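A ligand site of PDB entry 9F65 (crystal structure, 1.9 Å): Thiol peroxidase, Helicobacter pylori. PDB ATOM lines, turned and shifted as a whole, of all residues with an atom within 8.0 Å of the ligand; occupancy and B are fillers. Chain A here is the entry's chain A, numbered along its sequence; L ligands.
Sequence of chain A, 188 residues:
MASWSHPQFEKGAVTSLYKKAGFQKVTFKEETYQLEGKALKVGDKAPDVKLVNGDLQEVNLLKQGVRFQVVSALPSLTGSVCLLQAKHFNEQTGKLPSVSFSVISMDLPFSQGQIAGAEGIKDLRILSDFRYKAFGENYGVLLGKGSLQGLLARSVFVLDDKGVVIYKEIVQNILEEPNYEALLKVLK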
ATOM      1  N   PHE A  28     -13.760   0.764  -5.884  1.00  0.00           N
ATOM      2  CA  PHE A  28     -13.661  -0.636  -6.350  1.00  0.00           C
ATOM      3  C   PHE A  28     -12.274  -1.157  -5.998  1.00  0.00           C
ATOM      4  O   PHE A  28     -11.327  -0.828  -6.738  1.00  0.00           O
ATOM      5  CB  PHE A  28     -13.940  -0.734  -7.850  1.00  0.00           C
ATOM      6  CG  PHE A  28     -13.923  -2.134  -8.375  1.00  0.00           C
ATOM      7  CD1 PHE A  28     -13.257  -2.454  -9.555  1.00  0.00           C
ATOM      8  CD2 PHE A  28     -14.546  -3.151  -7.683  1.00  0.00           C
ATOM      9  CE1 PHE A  28     -13.257  -3.754 -10.028  1.00  0.00           C
ATOM     10  CE2 PHE A  28     -14.546  -4.451  -8.157  1.00  0.00           C
ATOM     11  CZ  PHE A  28     -13.906  -4.747  -9.333  1.00  0.00           C
ATOM     12  N   LYS A  29     -12.164  -1.895  -4.894  1.00  0.00           N
ATOM     13  CA  LYS A  29     -10.869  -2.389  -4.343  1.00  0.00           C
ATOM     14  C   LYS A  29      -9.949  -1.178  -4.165  1.00  0.00           C
ATOM     15  O   LYS A  29     -10.264  -0.350  -3.309  1.00  0.00           O
ATOM     16  CB  LYS A  29     -10.315  -3.481  -5.255  1.00  0.00           C
ATOM     17  CG  LYS A  29     -11.052  -4.809  -5.151  1.00  0.00           C
ATOM     18  CD  LYS A  29     -10.954  -5.684  -6.392  1.00  0.00           C
ATOM     19  CE  LYS A  29     -11.172  -7.149  -6.067  1.00  0.00           C
ATOM     20  NZ  LYS A  29     -11.901  -7.844  -7.153  1.00  0.00           N
ATOM     21  N   LEU A  74     -26.073  -0.990 -13.154  1.00  0.00           N
ATOM     22  CA  LEU A  74     -24.944  -1.778 -12.638  1.00  0.00           C
ATOM     23  C   LEU A  74     -23.879  -1.878 -13.727  1.00  0.00           C
ATOM     24  O   LEU A  74     -24.224  -1.723 -14.870  1.00  0.00           O
ATOM     25  CB  LEU A  74     -25.455  -3.159 -12.206  1.00  0.00           C
ATOM     26  CG  LEU A  74     -26.421  -3.805 -13.180  1.00  0.00           C
ATOM     27  CD1 LEU A  74     -25.662  -4.443 -14.324  1.00  0.00           C
ATOM     28  CD2 LEU A  74     -27.279  -4.829 -12.481  1.00  0.00           C
ATOM     29  N   PRO A  75     -22.609  -2.137 -13.390  1.00  0.00           N
ATOM     30  CA  PRO A  75     -21.528  -2.221 -14.367  1.00  0.00           C
ATOM     31  C   PRO A  75     -21.764  -3.266 -15.450  1.00  0.00           C
ATOM     32  O   PRO A  75     -21.645  -2.928 -16.575  1.00  0.00           O
ATOM     33  CB  PRO A  75     -20.307  -2.573 -13.524  1.00  0.00           C
ATOM     34  CG  PRO A  75     -20.666  -2.128 -12.135  1.00  0.00           C
ATOM     35  CD  PRO A  75     -22.145  -2.362 -12.035  1.00  0.00           C
ATOM     36  N   SER A  76     -22.106  -4.497 -15.068  1.00  0.00           N
ATOM     37  CA  SER A  76     -22.352  -5.578 -16.056  1.00  0.00           C
ATOM     38  C   SER A  76     -23.124  -6.739 -15.408  1.00  0.00           C
ATOM     39  O   SER A  76     -22.809  -7.068 -14.294  1.00  0.00           O
ATOM     40  CB  SER A  76     -21.053  -6.085 -16.612  1.00  0.00           C
ATOM     41  OG  SER A  76     -21.285  -7.142 -17.502  1.00  0.00           O
ATOM     42  N   LEU A  77     -24.069  -7.330 -16.136  1.00  0.00           N
ATOM     43  CA  LEU A  77     -24.870  -8.497 -15.679  1.00  0.00           C
ATOM     44  C   LEU A  77     -24.007  -9.767 -15.628  1.00  0.00           C
ATOM     45  O   LEU A  77     -24.503 -10.766 -15.077  1.00  0.00           O
ATOM     46  CB  LEU A  77     -26.053  -8.704 -16.633  1.00  0.00           C
ATOM     47  CG  LEU A  77     -27.212  -7.713 -16.494  1.00  0.00           C
ATOM     48  CD1 LEU A  77     -28.265  -8.009 -17.554  1.00  0.00           C
ATOM     49  CD2 LEU A  77     -27.821  -7.782 -15.097  1.00  0.00           C
ATOM     50  N   THR A  78     -22.778  -9.737 -16.158  1.00  0.00           N
ATOM     51  CA  THR A  78     -21.813 -10.877 -16.121  1.00  0.00           C
ATOM     52  C   THR A  78     -21.348 -11.141 -14.687  1.00  0.00           C
ATOM     53  O   THR A  78     -20.948 -12.284 -14.412  1.00  0.00           O
ATOM     54  CB  THR A  78     -20.613 -10.618 -17.041  1.00  0.00           C
ATOM     55  OG1 THR A  78     -19.903  -9.460 -16.599  1.00  0.00           O
ATOM     56  CG2 THR A  78     -20.998 -10.435 -18.495  1.00  0.00           C
ATOM     57  N   GLY A  79     -21.385 -10.133 -13.812  1.00  0.00           N
ATOM     58  CA  GLY A  79     -20.821 -10.183 -12.448  1.00  0.00           C
ATOM     59  C   GLY A  79     -21.818 -10.742 -11.443  1.00  0.00           C
ATOM     60  O   GLY A  79     -23.023 -10.494 -11.612  1.00  0.00           O
ATOM     61  N   SER A  80     -21.293 -11.454 -10.458  1.00  0.00           N
ATOM     62  CA  SER A  80     -22.105 -12.137  -9.415  1.00  0.00           C
ATOM     63  C   SER A  80     -22.945 -11.128  -8.628  1.00  0.00           C
ATOM     64  O   SER A  80     -24.143 -11.311  -8.553  1.00  0.00           O
ATOM     65  CB  SER A  80     -21.236 -12.934  -8.508  1.00  0.00           C
ATOM     66  OG  SER A  80     -20.328 -12.083  -7.831  1.00  0.00           O
ATOM     67  N   VAL A  81     -22.328 -10.089  -8.086  1.00  0.00           N
ATOM     68  CA  VAL A  81     -23.084  -9.062  -7.324  1.00  0.00           C
ATOM     69  C   VAL A  81     -24.133  -8.433  -8.242  1.00  0.00           C
ATOM     70  O   VAL A  81     -25.247  -8.244  -7.808  1.00  0.00           O
ATOM     71  CB  VAL A  81     -22.157  -7.993  -6.739  1.00  0.00           C
ATOM     72  CG1 VAL A  81     -22.955  -6.809  -6.244  1.00  0.00           C
ATOM     73  CG2 VAL A  81     -21.281  -8.559  -5.641  1.00  0.00           C
ATOM     74  N   CYS A  82     -23.752  -8.116  -9.481  1.00  0.00           N
ATOM     75  CA  CYS A  82     -24.636  -7.549 -10.444  1.00  0.00           C
ATOM     76  C   CYS A  82     -25.850  -8.439 -10.691  1.00  0.00           C
ATOM     77  O   CYS A  82     -26.955  -7.953 -10.770  1.00  0.00           O
ATOM     78  CB  CYS A  82     -23.848  -7.325 -11.712  1.00  0.00           C
ATOM     79  SG  CYS A  82     -22.749  -5.883 -11.642  1.00  0.00           S
ATOM     80  N   LEU A  83     -25.637  -9.754 -10.794  1.00  0.00           N
ATOM     81  CA  LEU A  83     -26.723 -10.722 -11.081  1.00  0.00           C
ATOM     82  C   LEU A  83     -27.682 -10.842  -9.897  1.00  0.00           C
ATOM     83  O   LEU A  83     -28.860 -11.010 -10.118  1.00  0.00           O
ATOM     84  CB  LEU A  83     -26.110 -12.071 -11.438  1.00  0.00           C
ATOM     85  CG  LEU A  83     -27.063 -13.064 -12.076  1.00  0.00           C
ATOM     86  CD1 LEU A  83     -27.564 -12.548 -13.406  1.00  0.00           C
ATOM     87  CD2 LEU A  83     -26.389 -14.413 -12.258  1.00  0.00           C
ATOM     88  N   LEU A  84     -27.155 -10.800  -8.689  1.00  0.00           N
ATOM     89  CA  LEU A  84     -27.999 -10.812  -7.462  1.00  0.00           C
ATOM     90  C   LEU A  84     -28.926  -9.582  -7.484  1.00  0.00           C
ATOM     91  O   LEU A  84     -30.115  -9.729  -7.165  1.00  0.00           O
ATOM     92  CB  LEU A  84     -27.101 -10.829  -6.217  1.00  0.00           C
ATOM     93  CG  LEU A  84     -26.363 -12.137  -5.948  1.00  0.00           C
ATOM     94  CD1 LEU A  84     -25.367 -11.976  -4.811  1.00  0.00           C
ATOM     95  CD2 LEU A  84     -27.327 -13.282  -5.649  1.00  0.00           C
ATOM     96  N   GLN A  85     -28.409  -8.422  -7.891  1.00  0.00           N
ATOM     97  CA  GLN A  85     -29.199  -7.176  -7.989  1.00  0.00           C
ATOM     98  C   GLN A  85     -30.326  -7.369  -9.019  1.00  0.00           C
ATOM     99  O   GLN A  85     -31.486  -7.011  -8.705  1.00  0.00           O
ATOM    100  CB  GLN A  85     -28.292  -6.004  -8.350  1.00  0.00           C
ATOM    101  CG  GLN A  85     -29.005  -4.680  -8.561  1.00  0.00           C
ATOM    102  CD  GLN A  85     -27.996  -3.616  -8.900  1.00  0.00           C
ATOM    103  OE1 GLN A  85     -26.802  -3.793  -8.670  1.00  0.00           O
ATOM    104  NE2 GLN A  85     -28.463  -2.520  -9.462  1.00  0.00           N
ATOM    105  N   ASP A 107     -23.825  -3.430 -21.051  1.00  0.00           N
ATOM    106  CA  ASP A 107     -23.892  -4.723 -21.788  1.00  0.00           C
ATOM    107  C   ASP A 107     -24.757  -4.515 -23.030  1.00  0.00           C
ATOM    108  O   ASP A 107     -25.832  -3.868 -22.900  1.00  0.00           O
ATOM    109  CB  ASP A 107     -24.503  -5.839 -20.940  1.00  0.00           C
ATOM    110  CG  ASP A 107     -23.797  -6.112 -19.623  1.00  0.00           C
ATOM    111  OD1 ASP A 107     -22.685  -6.667 -19.656  1.00  0.00           O
ATOM    112  OD2 ASP A 107     -24.368  -5.779 -18.567  1.00  0.00           O
ATOM    113  N   LEU A 148     -12.974   0.299 -14.707  1.00  0.00           N
ATOM    114  CA  LEU A 148     -14.446   0.232 -14.977  1.00  0.00           C
ATOM    115  C   LEU A 148     -14.928   1.447 -15.771  1.00  0.00           C
ATOM    116  O   LEU A 148     -16.156   1.612 -15.901  1.00  0.00           O
ATOM    117  CB  LEU A 148     -15.194   0.126 -13.640  1.00  0.00           C
ATOM    118  CG  LEU A 148     -14.892  -1.092 -12.774  1.00  0.00           C
ATOM    119  CD1 LEU A 148     -15.676  -1.016 -11.472  1.00  0.00           C
ATOM    120  CD2 LEU A 148     -15.203  -2.392 -13.509  1.00  0.00           C
ATOM    121  N   LEU A 151     -18.462   2.262 -17.722  1.00  0.00           N
ATOM    122  CA  LEU A 151     -19.532   1.386 -17.175  1.00  0.00           C
ATOM    123  C   LEU A 151     -20.397   2.228 -16.227  1.00  0.00           C
ATOM    124  O   LEU A 151     -19.957   3.330 -15.858  1.00  0.00           O
ATOM    125  CB  LEU A 151     -18.904   0.175 -16.474  1.00  0.00           C
ATOM    126  CG  LEU A 151     -18.049  -0.729 -17.368  1.00  0.00           C
ATOM    127  CD1 LEU A 151     -17.552  -1.949 -16.600  1.00  0.00           C
ATOM    128  CD2 LEU A 151     -18.814  -1.170 -18.608  1.00  0.00           C
ATOM    129  N   LEU A 152     -21.591   1.761 -15.881  1.00  0.00           N
ATOM    130  CA  LEU A 152     -22.492   2.509 -14.970  1.00  0.00           C
ATOM    131  C   LEU A 152     -22.234   2.094 -13.519  1.00  0.00           C
ATOM    132  O   LEU A 152     -22.113   0.873 -13.260  1.00  0.00           O
ATOM    133  CB  LEU A 152     -23.955   2.278 -15.377  1.00  0.00           C
ATOM    134  CG  LEU A 152     -24.303   2.653 -16.813  1.00  0.00           C
ATOM    135  CD1 LEU A 152     -25.723   2.248 -17.137  1.00  0.00           C
ATOM    136  CD2 LEU A 152     -24.110   4.139 -17.074  1.00  0.00           C
ATOM    137  N   ARG A 154     -23.119   1.250  -9.745  1.00  0.00           N
ATOM    138  CA  ARG A 154     -24.257   0.572  -9.079  1.00  0.00           C
ATOM    139  C   ARG A 154     -25.086   1.645  -8.391  1.00  0.00           C
ATOM    140  O   ARG A 154     -24.528   2.422  -7.608  1.00  0.00           O
ATOM    141  CB  ARG A 154     -23.784  -0.491  -8.087  1.00  0.00           C
ATOM    142  CG  ARG A 154     -24.918  -1.394  -7.630  1.00  0.00           C
ATOM    143  CD  ARG A 154     -24.503  -2.464  -6.658  1.00  0.00           C
ATOM    144  NE  ARG A 154     -23.223  -3.067  -6.983  1.00  0.00           N
ATOM    145  CZ  ARG A 154     -22.975  -3.838  -8.042  1.00  0.00           C
ATOM    146  NH1 ARG A 154     -23.926  -4.116  -8.919  1.00  0.00           N
ATOM    147  NH2 ARG A 154     -21.769  -4.342  -8.219  1.00  0.00           N
ATOM    148  N   ASN A 173     -19.244   1.511  -2.184  1.00  0.00           N
ATOM    149  CA  ASN A 173     -18.390   0.339  -2.497  1.00  0.00           C
ATOM    150  C   ASN A 173     -19.137  -0.526  -3.512  1.00  0.00           C
ATOM    151  O   ASN A 173     -20.143  -1.138  -3.134  1.00  0.00           O
ATOM    152  CB  ASN A 173     -18.024  -0.449  -1.237  1.00  0.00           C
ATOM    153  CG  ASN A 173     -17.223  -1.703  -1.517  1.00  0.00           C
ATOM    154  OD1 ASN A 173     -16.844  -1.981  -2.660  1.00  0.00           O
ATOM    155  ND2 ASN A 173     -16.946  -2.487  -0.484  1.00  0.00           N
ATOM    156  N   ILE A 174     -18.636  -0.595  -4.744  1.00  0.00           N
ATOM    157  CA  ILE A 174     -19.350  -1.220  -5.894  1.00  0.00           C
ATOM    158  C   ILE A 174     -19.431  -2.745  -5.689  1.00  0.00           C
ATOM    159  O   ILE A 174     -20.247  -3.373  -6.382  1.00  0.00           O
ATOM    160  CB  ILE A 174     -18.678  -0.811  -7.219  1.00  0.00           C
ATOM    161  CG1 ILE A 174     -19.689  -0.728  -8.367  1.00  0.00           C
ATOM    162  CG2 ILE A 174     -17.513  -1.719  -7.548  1.00  0.00           C
ATOM    163  CD1 ILE A 174     -19.163   0.007  -9.573  1.00  0.00           C
ATOM    164  N   LEU A 175     -18.652  -3.308  -4.764  1.00  0.00           N
ATOM    165  CA  LEU A 175     -18.729  -4.744  -4.364  1.00  0.00           C
ATOM    166  C   LEU A 175     -19.942  -5.004  -3.462  1.00  0.00           C
ATOM    167  O   LEU A 175     -20.252  -6.190  -3.235  1.00  0.00           O
ATOM    168  CB  LEU A 175     -17.433  -5.162  -3.651  1.00  0.00           C
ATOM    169  CG  LEU A 175     -16.188  -5.257  -4.533  1.00  0.00           C
ATOM    170  CD1 LEU A 175     -14.950  -5.497  -3.679  1.00  0.00           C
ATOM    171  CD2 LEU A 175     -16.347  -6.363  -5.570  1.00  0.00           C
ATOM    172  N   GLU A 176     -20.573  -3.953  -2.938  1.00  0.00           N
ATOM    173  CA  GLU A 176     -21.796  -4.059  -2.097  1.00  0.00           C
ATOM    174  C   GLU A 176     -23.031  -4.091  -2.999  1.00  0.00           C
ATOM    175  O   GLU A 176     -23.006  -3.429  -4.056  1.00  0.00           O
ATOM    176  CB  GLU A 176     -21.919  -2.877  -1.131  1.00  0.00           C
ATOM    177  CG  GLU A 176     -20.757  -2.747  -0.161  1.00  0.00           C
ATOM    178  CD  GLU A 176     -20.887  -3.524   1.140  1.00  0.00           C
ATOM    179  OE1 GLU A 176     -20.050  -3.305   2.033  1.00  0.00           O
ATOM    180  OE2 GLU A 176     -21.830  -4.345   1.245  1.00  0.00           O
HETATM  181  C1  LIG L   1     -21.337  -6.387 -11.092  1.00  0.00           C
HETATM  182  C2  LIG L   1     -20.304  -6.841 -11.788  1.00  0.00           C
HETATM  183  C3  LIG L   1     -19.747  -6.795  -9.790  1.00  0.00           C
HETATM  184  N1  LIG L   1     -20.165  -7.037 -13.074  1.00  0.00           N
HETATM  185  C4  LIG L   1     -18.923  -6.947  -8.537  1.00  0.00           C
HETATM  186  C5  LIG L   1     -19.326  -9.281  -9.043  1.00  0.00           C
HETATM  187  C6  LIG L   1     -18.430 -10.113  -9.706  1.00  0.00           C
HETATM  188  N2  LIG L   1     -20.975  -6.354  -9.837  1.00  0.00           N
HETATM  189  N3  LIG L   1     -19.317  -7.105 -10.980  1.00  0.00           N
HETATM  190  C7  LIG L   1     -17.992  -7.642 -11.303  1.00  0.00           C
HETATM  191  O1  LIG L   1     -18.628  -8.324  -8.262  1.00  0.00           O
HETATM  192  C8  LIG L   1     -17.717 -10.788 -10.248  1.00  0.00           C
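The backbone NH (N) of Cys 82 is in hydrogen-bond range of a nitrogen (N2) of the ligand (3.3 Å).
SG of Cys 82 is covalently linked to C1 of the ligand, at 1.6 Å.
N2 of the ligand is in hydrogen-bond range of NH2 of Arg 154.
N1 of the ligand sits at hydrogen-bond distance from O of Ser 76, 2.9 Å away.
The side-chain sulfur (SG) of Cys 82 sits at hydrogen-bond distance from the guanidinium group (NH1) of Arg 154.
The side-chain sulfur (SG) of Cys 82 lies within hydrogen-bond range of the backbone NH (N) of Ser 76 (3.8 Å).
NH2 of Arg 154 lies within hydrogen-bond range of O of Ile 174, at 2.6 Å.
The side-chain amide oxygen (OE1) of Gln 85 lies within hydrogen-bond range of the guanidinium group (NH1) of Arg 154.
O of Glu 176 sits at hydrogen-bond distance from NE of Arg 154 (3.0 Å).
OG of Ser 76 is in hydrogen-bond range of OG1 of Thr 78.
OG of Ser 76 lies within hydrogen-bond range of OD1 of Asp 107, at 2.6 Å.
The backbone NH (N) of Leu 175 sits at hydrogen-bond distance from the side-chain amide oxygen (OD1) of Asn 173 (3.1 Å).
N of Gly 79 sits close to N1 of the ligand (3.4 Å).
Ser 80 touches the ligand.
N of Val 81 touches C5 of the ligand (3.3 Å).
Leu 175 touches the ligand (CD2 to C4, 3.97 Å).
Hydrophobic or aromatic side chains that line the ligand: Val 81 and Leu 175.
Within 4 Å of the ligand: Ser 76, Gly 79, Ser 80, Val 81, Cys 82, Arg 154 and Leu 175.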
